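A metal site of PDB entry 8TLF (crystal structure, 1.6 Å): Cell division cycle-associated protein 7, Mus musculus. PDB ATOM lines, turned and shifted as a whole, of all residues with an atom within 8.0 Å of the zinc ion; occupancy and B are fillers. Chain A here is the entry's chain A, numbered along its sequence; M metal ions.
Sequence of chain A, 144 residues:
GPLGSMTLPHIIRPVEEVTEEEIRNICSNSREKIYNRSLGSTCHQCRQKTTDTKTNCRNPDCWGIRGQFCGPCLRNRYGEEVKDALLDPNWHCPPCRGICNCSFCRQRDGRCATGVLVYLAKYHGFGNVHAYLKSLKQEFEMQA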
ATOM      1  N   HIS A  10       7.531 -17.245 -28.956  1.00  0.00           N
ATOM      2  CA  HIS A  10       6.721 -18.164 -28.184  1.00  0.00           C
ATOM      3  C   HIS A  10       7.095 -18.027 -26.714  1.00  0.00           C
ATOM      4  O   HIS A  10       8.262 -18.202 -26.341  1.00  0.00           O
ATOM      5  CB  HIS A  10       6.925 -19.609 -28.660  1.00  0.00           C
ATOM      6  CG  HIS A  10       6.256 -20.622 -27.796  1.00  0.00           C
ATOM      7  ND1 HIS A  10       6.970 -21.536 -27.034  1.00  0.00           N
ATOM      8  CD2 HIS A  10       4.951 -20.881 -27.558  1.00  0.00           C
ATOM      9  CE1 HIS A  10       6.122 -22.309 -26.372  1.00  0.00           C
ATOM     10  NE2 HIS A  10       4.898 -21.936 -26.674  1.00  0.00           N
ATOM     11  N   ASN A  56      -1.884 -22.771 -24.784  1.00  0.00           N
ATOM     12  CA  ASN A  56      -0.493 -22.328 -24.766  1.00  0.00           C
ATOM     13  C   ASN A  56       0.395 -23.569 -24.684  1.00  0.00           C
ATOM     14  O   ASN A  56       0.419 -24.247 -23.659  1.00  0.00           O
ATOM     15  CB  ASN A  56      -0.230 -21.384 -23.602  1.00  0.00           C
ATOM     16  CG  ASN A  56       1.238 -21.002 -23.475  1.00  0.00           C
ATOM     17  OD1 ASN A  56       1.969 -21.556 -22.653  1.00  0.00           O
ATOM     18  ND2 ASN A  56       1.673 -20.049 -24.288  1.00  0.00           N
ATOM     19  N   CYS A  57       1.121 -23.859 -25.765  1.00  0.00           N
ATOM     20  CA  CYS A  57       2.011 -25.007 -25.771  1.00  0.00           C
ATOM     21  C   CYS A  57       3.189 -24.765 -24.833  1.00  0.00           C
ATOM     22  O   CYS A  57       3.838 -23.718 -24.903  1.00  0.00           O
ATOM     23  CB  CYS A  57       2.509 -25.297 -27.186  1.00  0.00           C
ATOM     24  SG  CYS A  57       3.536 -26.787 -27.317  1.00  0.00           S
ATOM     25  N   ARG A  58       3.453 -25.721 -23.958  1.00  0.00           N
ATOM     26  CA  ARG A  58       4.518 -25.596 -22.962  1.00  0.00           C
ATOM     27  C   ARG A  58       5.763 -26.389 -23.336  1.00  0.00           C
ATOM     28  O   ARG A  58       6.642 -26.577 -22.488  1.00  0.00           O
ATOM     29  CB  ARG A  58       3.995 -26.018 -21.586  1.00  0.00           C
ATOM     30  CG  ARG A  58       2.898 -25.099 -21.079  1.00  0.00           C
ATOM     31  CD  ARG A  58       2.465 -25.442 -19.665  1.00  0.00           C
ATOM     32  NE  ARG A  58       1.563 -24.422 -19.141  1.00  0.00           N
ATOM     33  CZ  ARG A  58       0.245 -24.404 -19.328  1.00  0.00           C
ATOM     34  NH1 ARG A  58      -0.356 -25.360 -20.016  1.00  0.00           N
ATOM     35  NH2 ARG A  58      -0.469 -23.413 -18.816  1.00  0.00           N
ATOM     36  N   ASN A  59       5.859 -26.853 -24.578  1.00  0.00           N
ATOM     37  CA  ASN A  59       7.082 -27.463 -25.057  1.00  0.00           C
ATOM     38  C   ASN A  59       8.102 -26.370 -25.378  1.00  0.00           C
ATOM     39  O   ASN A  59       7.809 -25.479 -26.180  1.00  0.00           O
ATOM     40  CB  ASN A  59       6.815 -28.302 -26.307  1.00  0.00           C
ATOM     41  CG  ASN A  59       8.063 -28.971 -26.846  1.00  0.00           C
ATOM     42  OD1 ASN A  59       9.025 -29.211 -26.120  1.00  0.00           O
ATOM     43  ND2 ASN A  59       8.044 -29.279 -28.142  1.00  0.00           N
ATOM     44  N   PRO A  60       9.287 -26.385 -24.760  1.00  0.00           N
ATOM     45  CA  PRO A  60      10.278 -25.339 -25.066  1.00  0.00           C
ATOM     46  C   PRO A  60      10.711 -25.332 -26.517  1.00  0.00           C
ATOM     47  O   PRO A  60      11.136 -24.283 -27.023  1.00  0.00           O
ATOM     48  CB  PRO A  60      11.446 -25.692 -24.131  1.00  0.00           C
ATOM     49  CG  PRO A  60      10.829 -26.481 -23.026  1.00  0.00           C
ATOM     50  CD  PRO A  60       9.716 -27.263 -23.658  1.00  0.00           C
ATOM     51  N   ASP A  61      10.618 -26.456 -27.218  1.00  0.00           N
ATOM     52  CA  ASP A  61      11.018 -26.530 -28.620  1.00  0.00           C
ATOM     53  C   ASP A  61       9.956 -26.002 -29.564  1.00  0.00           C
ATOM     54  O   ASP A  61      10.207 -25.916 -30.774  1.00  0.00           O
ATOM     55  CB  ASP A  61      11.361 -27.977 -28.990  1.00  0.00           C
ATOM     56  CG  ASP A  61      12.503 -28.528 -28.153  1.00  0.00           C
ATOM     57  OD1 ASP A  61      13.362 -27.727 -27.720  1.00  0.00           O
ATOM     58  OD2 ASP A  61      12.552 -29.762 -27.945  1.00  0.00           O
ATOM     59  N   CYS A  62       8.773 -25.652 -29.063  1.00  0.00           N
ATOM     60  CA  CYS A  62       7.737 -25.081 -29.911  1.00  0.00           C
ATOM     61  C   CYS A  62       8.097 -23.644 -30.278  1.00  0.00           C
ATOM     62  O   CYS A  62       8.947 -23.003 -29.645  1.00  0.00           O
ATOM     63  CB  CYS A  62       6.385 -25.123 -29.206  1.00  0.00           C
ATOM     64  SG  CYS A  62       4.954 -24.950 -30.307  1.00  0.00           S
ATOM     65  N   TRP A  63       7.453 -23.141 -31.323  1.00  0.00           N
ATOM     66  CA  TRP A  63       7.735 -21.796 -31.811  1.00  0.00           C
ATOM     67  C   TRP A  63       6.479 -21.217 -32.447  1.00  0.00           C
ATOM     68  O   TRP A  63       5.593 -21.947 -32.900  1.00  0.00           O
ATOM     69  CB  TRP A  63       8.895 -21.788 -32.807  1.00  0.00           C
ATOM     70  CG  TRP A  63       8.536 -22.401 -34.132  1.00  0.00           C
ATOM     71  CD1 TRP A  63       8.162 -21.747 -35.268  1.00  0.00           C
ATOM     72  CD2 TRP A  63       8.515 -23.798 -34.450  1.00  0.00           C
ATOM     73  NE1 TRP A  63       7.908 -22.653 -36.266  1.00  0.00           N
ATOM     74  CE2 TRP A  63       8.122 -23.916 -35.796  1.00  0.00           C
ATOM     75  CE3 TRP A  63       8.797 -24.964 -33.727  1.00  0.00           C
ATOM     76  CZ2 TRP A  63       8.001 -25.145 -36.440  1.00  0.00           C
ATOM     77  CZ3 TRP A  63       8.676 -26.195 -34.361  1.00  0.00           C
ATOM     78  CH2 TRP A  63       8.282 -26.273 -35.701  1.00  0.00           C
ATOM     79  N   GLY A  64       6.430 -19.889 -32.500  1.00  0.00           N
ATOM     80  CA  GLY A  64       5.325 -19.214 -33.169  1.00  0.00           C
ATOM     81  C   GLY A  64       4.000 -19.428 -32.459  1.00  0.00           C
ATOM     82  O   GLY A  64       3.909 -19.580 -31.244  1.00  0.00           O
ATOM     83  N   ILE A  65       2.929 -19.442 -33.268  1.00  0.00           N
ATOM     84  CA  ILE A  65       1.567 -19.569 -32.767  1.00  0.00           C
ATOM     85  C   ILE A  65       0.960 -20.919 -33.115  1.00  0.00           C
ATOM     86  O   ILE A  65      -0.263 -21.086 -32.999  1.00  0.00           O
ATOM     87  CB  ILE A  65       0.681 -18.424 -33.287  1.00  0.00           C
ATOM     88  CG1 ILE A  65       0.500 -18.545 -34.803  1.00  0.00           C
ATOM     89  CG2 ILE A  65       1.288 -17.075 -32.928  1.00  0.00           C
ATOM     90  CD1 ILE A  65      -0.594 -17.661 -35.352  1.00  0.00           C
ATOM     91  N   ARG A  66       1.777 -21.882 -33.547  1.00  0.00           N
ATOM     92  CA  ARG A  66       1.248 -23.193 -33.924  1.00  0.00           C
ATOM     93  C   ARG A  66       0.591 -23.901 -32.744  1.00  0.00           C
ATOM     94  O   ARG A  66      -0.231 -24.801 -32.950  1.00  0.00           O
ATOM     95  CB  ARG A  66       2.362 -24.053 -34.514  1.00  0.00           C
ATOM     96  CG  ARG A  66       3.489 -24.372 -33.543  1.00  0.00           C
ATOM     97  CD  ARG A  66       4.778 -24.725 -34.271  1.00  0.00           C
ATOM     98  NE  ARG A  66       4.722 -26.028 -34.928  1.00  0.00           N
ATOM     99  CZ  ARG A  66       5.164 -27.153 -34.387  1.00  0.00           C
ATOM    100  NH1 ARG A  66       5.690 -27.189 -33.180  1.00  0.00           N
ATOM    101  NH2 ARG A  66       5.090 -28.282 -35.090  1.00  0.00           N
ATOM    102  N   GLY A  67       0.938 -23.520 -31.511  1.00  0.00           N
ATOM    103  CA  GLY A  67       0.384 -24.127 -30.322  1.00  0.00           C
ATOM    104  C   GLY A  67      -0.886 -23.514 -29.790  1.00  0.00           C
ATOM    105  O   GLY A  67      -1.358 -23.926 -28.728  1.00  0.00           O
ATOM    106  N   GLN A  68      -1.473 -22.542 -30.499  1.00  0.00           N
ATOM    107  CA  GLN A  68      -2.671 -21.852 -30.040  1.00  0.00           C
ATOM    108  C   GLN A  68      -3.893 -22.451 -30.713  1.00  0.00           C
ATOM    109  O   GLN A  68      -4.021 -22.415 -31.936  1.00  0.00           O
ATOM    110  CB  GLN A  68      -2.571 -20.358 -30.348  1.00  0.00           C
ATOM    111  CG  GLN A  68      -1.374 -19.664 -29.732  1.00  0.00           C
ATOM    112  CD  GLN A  68      -1.259 -18.214 -30.127  1.00  0.00           C
ATOM    113  OE1 GLN A  68      -2.076 -17.699 -30.901  1.00  0.00           O
ATOM    114  NE2 GLN A  68      -0.245 -17.529 -29.616  1.00  0.00           N
ATOM    115  N   PHE A  69      -4.807 -22.994 -29.894  1.00  0.00           N
ATOM    116  CA  PHE A  69      -6.047 -23.593 -30.374  1.00  0.00           C
ATOM    117  C   PHE A  69      -7.221 -23.046 -29.583  1.00  0.00           C
ATOM    118  O   PHE A  69      -7.147 -22.894 -28.362  1.00  0.00           O
ATOM    119  CB  PHE A  69      -6.004 -25.123 -30.259  1.00  0.00           C
ATOM    120  CG  PHE A  69      -5.080 -25.777 -31.247  1.00  0.00           C
ATOM    121  CD1 PHE A  69      -3.713 -25.818 -31.035  1.00  0.00           C
ATOM    122  CD2 PHE A  69      -5.586 -26.361 -32.401  1.00  0.00           C
ATOM    123  CE1 PHE A  69      -2.866 -26.425 -31.943  1.00  0.00           C
ATOM    124  CE2 PHE A  69      -4.741 -26.977 -33.311  1.00  0.00           C
ATOM    125  CZ  PHE A  69      -3.389 -26.997 -33.084  1.00  0.00           C
ATOM    126  N   TRP A  91       1.504 -29.985 -21.179  1.00  0.00           N
ATOM    127  CA  TRP A  91       0.693 -30.095 -22.385  1.00  0.00           C
ATOM    128  C   TRP A  91       1.487 -29.647 -23.617  1.00  0.00           C
ATOM    129  O   TRP A  91       2.114 -28.586 -23.603  1.00  0.00           O
ATOM    130  CB  TRP A  91      -0.578 -29.254 -22.246  1.00  0.00           C
ATOM    131  CG  TRP A  91      -1.531 -29.424 -23.394  1.00  0.00           C
ATOM    132  CD1 TRP A  91      -2.459 -30.412 -23.548  1.00  0.00           C
ATOM    133  CD2 TRP A  91      -1.642 -28.577 -24.544  1.00  0.00           C
ATOM    134  NE1 TRP A  91      -3.148 -30.233 -24.718  1.00  0.00           N
ATOM    135  CE2 TRP A  91      -2.667 -29.116 -25.357  1.00  0.00           C
ATOM    136  CE3 TRP A  91      -0.975 -27.425 -24.973  1.00  0.00           C
ATOM    137  CZ2 TRP A  91      -3.040 -28.536 -26.564  1.00  0.00           C
ATOM    138  CZ3 TRP A  91      -1.351 -26.854 -26.181  1.00  0.00           C
ATOM    139  CH2 TRP A  91      -2.367 -27.411 -26.957  1.00  0.00           C
ATOM    140  N   HIS A  92       1.452 -30.470 -24.662  1.00  0.00           N
ATOM    141  CA  HIS A  92       2.073 -30.153 -25.946  1.00  0.00           C
ATOM    142  C   HIS A  92       0.996 -30.060 -27.011  1.00  0.00           C
ATOM    143  O   HIS A  92       0.032 -30.823 -27.010  1.00  0.00           O
ATOM    144  CB  HIS A  92       3.109 -31.209 -26.338  1.00  0.00           C
ATOM    145  CG  HIS A  92       4.336 -31.205 -25.467  1.00  0.00           C
ATOM    146  ND1 HIS A  92       5.434 -32.002 -25.735  1.00  0.00           N
ATOM    147  CD2 HIS A  92       4.637 -30.510 -24.350  1.00  0.00           C
ATOM    148  CE1 HIS A  92       6.359 -31.786 -24.811  1.00  0.00           C
ATOM    149  NE2 HIS A  92       5.895 -30.893 -23.959  1.00  0.00           N
ATOM    150  N   CYS A  93       1.168 -29.108 -27.935  1.00  0.00           N
ATOM    151  CA  CYS A  93       0.188 -28.894 -28.977  1.00  0.00           C
ATOM    152  C   CYS A  93       0.200 -30.052 -29.980  1.00  0.00           C
ATOM    153  O   CYS A  93       1.202 -30.765 -30.101  1.00  0.00           O
ATOM    154  CB  CYS A  93       0.461 -27.567 -29.700  1.00  0.00           C
ATOM    155  SG  CYS A  93       1.998 -27.531 -30.656  1.00  0.00           S
ATOM    156  N   PRO A  94      -0.904 -30.258 -30.693  1.00  0.00           N
ATOM    157  CA  PRO A  94      -0.958 -31.342 -31.683  1.00  0.00           C
ATOM    158  C   PRO A  94       0.136 -31.240 -32.733  1.00  0.00           C
ATOM    159  O   PRO A  94       0.672 -32.276 -33.164  1.00  0.00           O
ATOM    160  CB  PRO A  94      -2.359 -31.176 -32.312  1.00  0.00           C
ATOM    161  CG  PRO A  94      -3.162 -30.573 -31.214  1.00  0.00           C
ATOM    162  CD  PRO A  94      -2.229 -29.666 -30.456  1.00  0.00           C
ATOM    163  N   PRO A  95       0.515 -30.032 -33.194  1.00  0.00           N
ATOM    164  CA  PRO A  95       1.699 -29.953 -34.059  1.00  0.00           C
ATOM    165  C   PRO A  95       2.961 -30.503 -33.419  1.00  0.00           C
ATOM    166  O   PRO A  95       3.750 -31.170 -34.091  1.00  0.00           O
ATOM    167  CB  PRO A  95       1.821 -28.455 -34.357  1.00  0.00           C
ATOM    168  CG  PRO A  95       0.430 -27.968 -34.314  1.00  0.00           C
ATOM    169  CD  PRO A  95      -0.214 -28.742 -33.195  1.00  0.00           C
ATOM    170  N   CYS A  96       3.172 -30.256 -32.129  1.00  0.00           N
ATOM    171  CA  CYS A  96       4.344 -30.804 -31.445  1.00  0.00           C
ATOM    172  C   CYS A  96       4.249 -32.317 -31.311  1.00  0.00           C
ATOM    173  O   CYS A  96       5.272 -33.004 -31.348  1.00  0.00           O
ATOM    174  CB  CYS A  96       4.520 -30.157 -30.076  1.00  0.00           C
ATOM    175  SG  CYS A  96       5.383 -28.573 -30.109  1.00  0.00           S
ATOM    176  N   ARG A  97       3.035 -32.852 -31.157  1.00  0.00           N
ATOM    177  CA  ARG A  97       2.828 -34.289 -31.099  1.00  0.00           C
ATOM    178  C   ARG A  97       2.738 -34.911 -32.487  1.00  0.00           C
ATOM    179  O   ARG A  97       2.633 -36.143 -32.587  1.00  0.00           O
ATOM    180  CB  ARG A  97       1.560 -34.598 -30.314  1.00  0.00           C
ATOM    181  CG  ARG A  97       1.701 -34.416 -28.808  1.00  0.00           C
ATOM    182  CD  ARG A  97       0.376 -34.629 -28.098  1.00  0.00           C
ATOM    183  NE  ARG A  97      -0.531 -33.506 -28.267  1.00  0.00           N
ATOM    184  CZ  ARG A  97      -1.782 -33.475 -27.808  1.00  0.00           C
ATOM    185  NH1 ARG A  97      -2.305 -34.501 -27.164  1.00  0.00           N
ATOM    186  NH2 ARG A  97      -2.512 -32.375 -28.008  1.00  0.00           N
HETATM  187 ZN    ZN M   1       3.887 -26.911 -29.582  1.00  0.00          ZN
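SG of Cys 93 binds the zinc ion.
The side-chain sulfur (SG) of Cys 57 is bound to the zinc ion.
SG of Cys 96 is bound to the zinc ion, at 2.3 Å.
The side-chain sulfur (SG) of Cys 62 is bound to the zinc ion, 2.3 Å away.
The zinc ion has four donor atoms within binding distance.
The backbone NH (N) of Asn 59 sits close to the side-chain sulfur (SG) of Cys 57, 3.6 Å away.
The backbone carbonyl oxygen (O) of Cys 57 lies within hydrogen-bond range of a ring nitrogen (NE2) of His 10.
The guanidinium group (NH1) of Arg 66 lies close to the side-chain sulfur (SG) of Cys 96 (3.4 Å).
SG of Cys 96 sits close to ND2 of Asn 59.
The side-chain sulfur (SG) of Cys 62 sits close to the guanidinium group (NH1) of Arg 66 (3.7 Å).
Four residues have an atom within 4 Å of the zinc ion: Cys 57, Cys 62, Cys 93 and Cys 96.
The nearest printed residue that does not touch the zinc ion is Arg 66 (4.03 Å).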
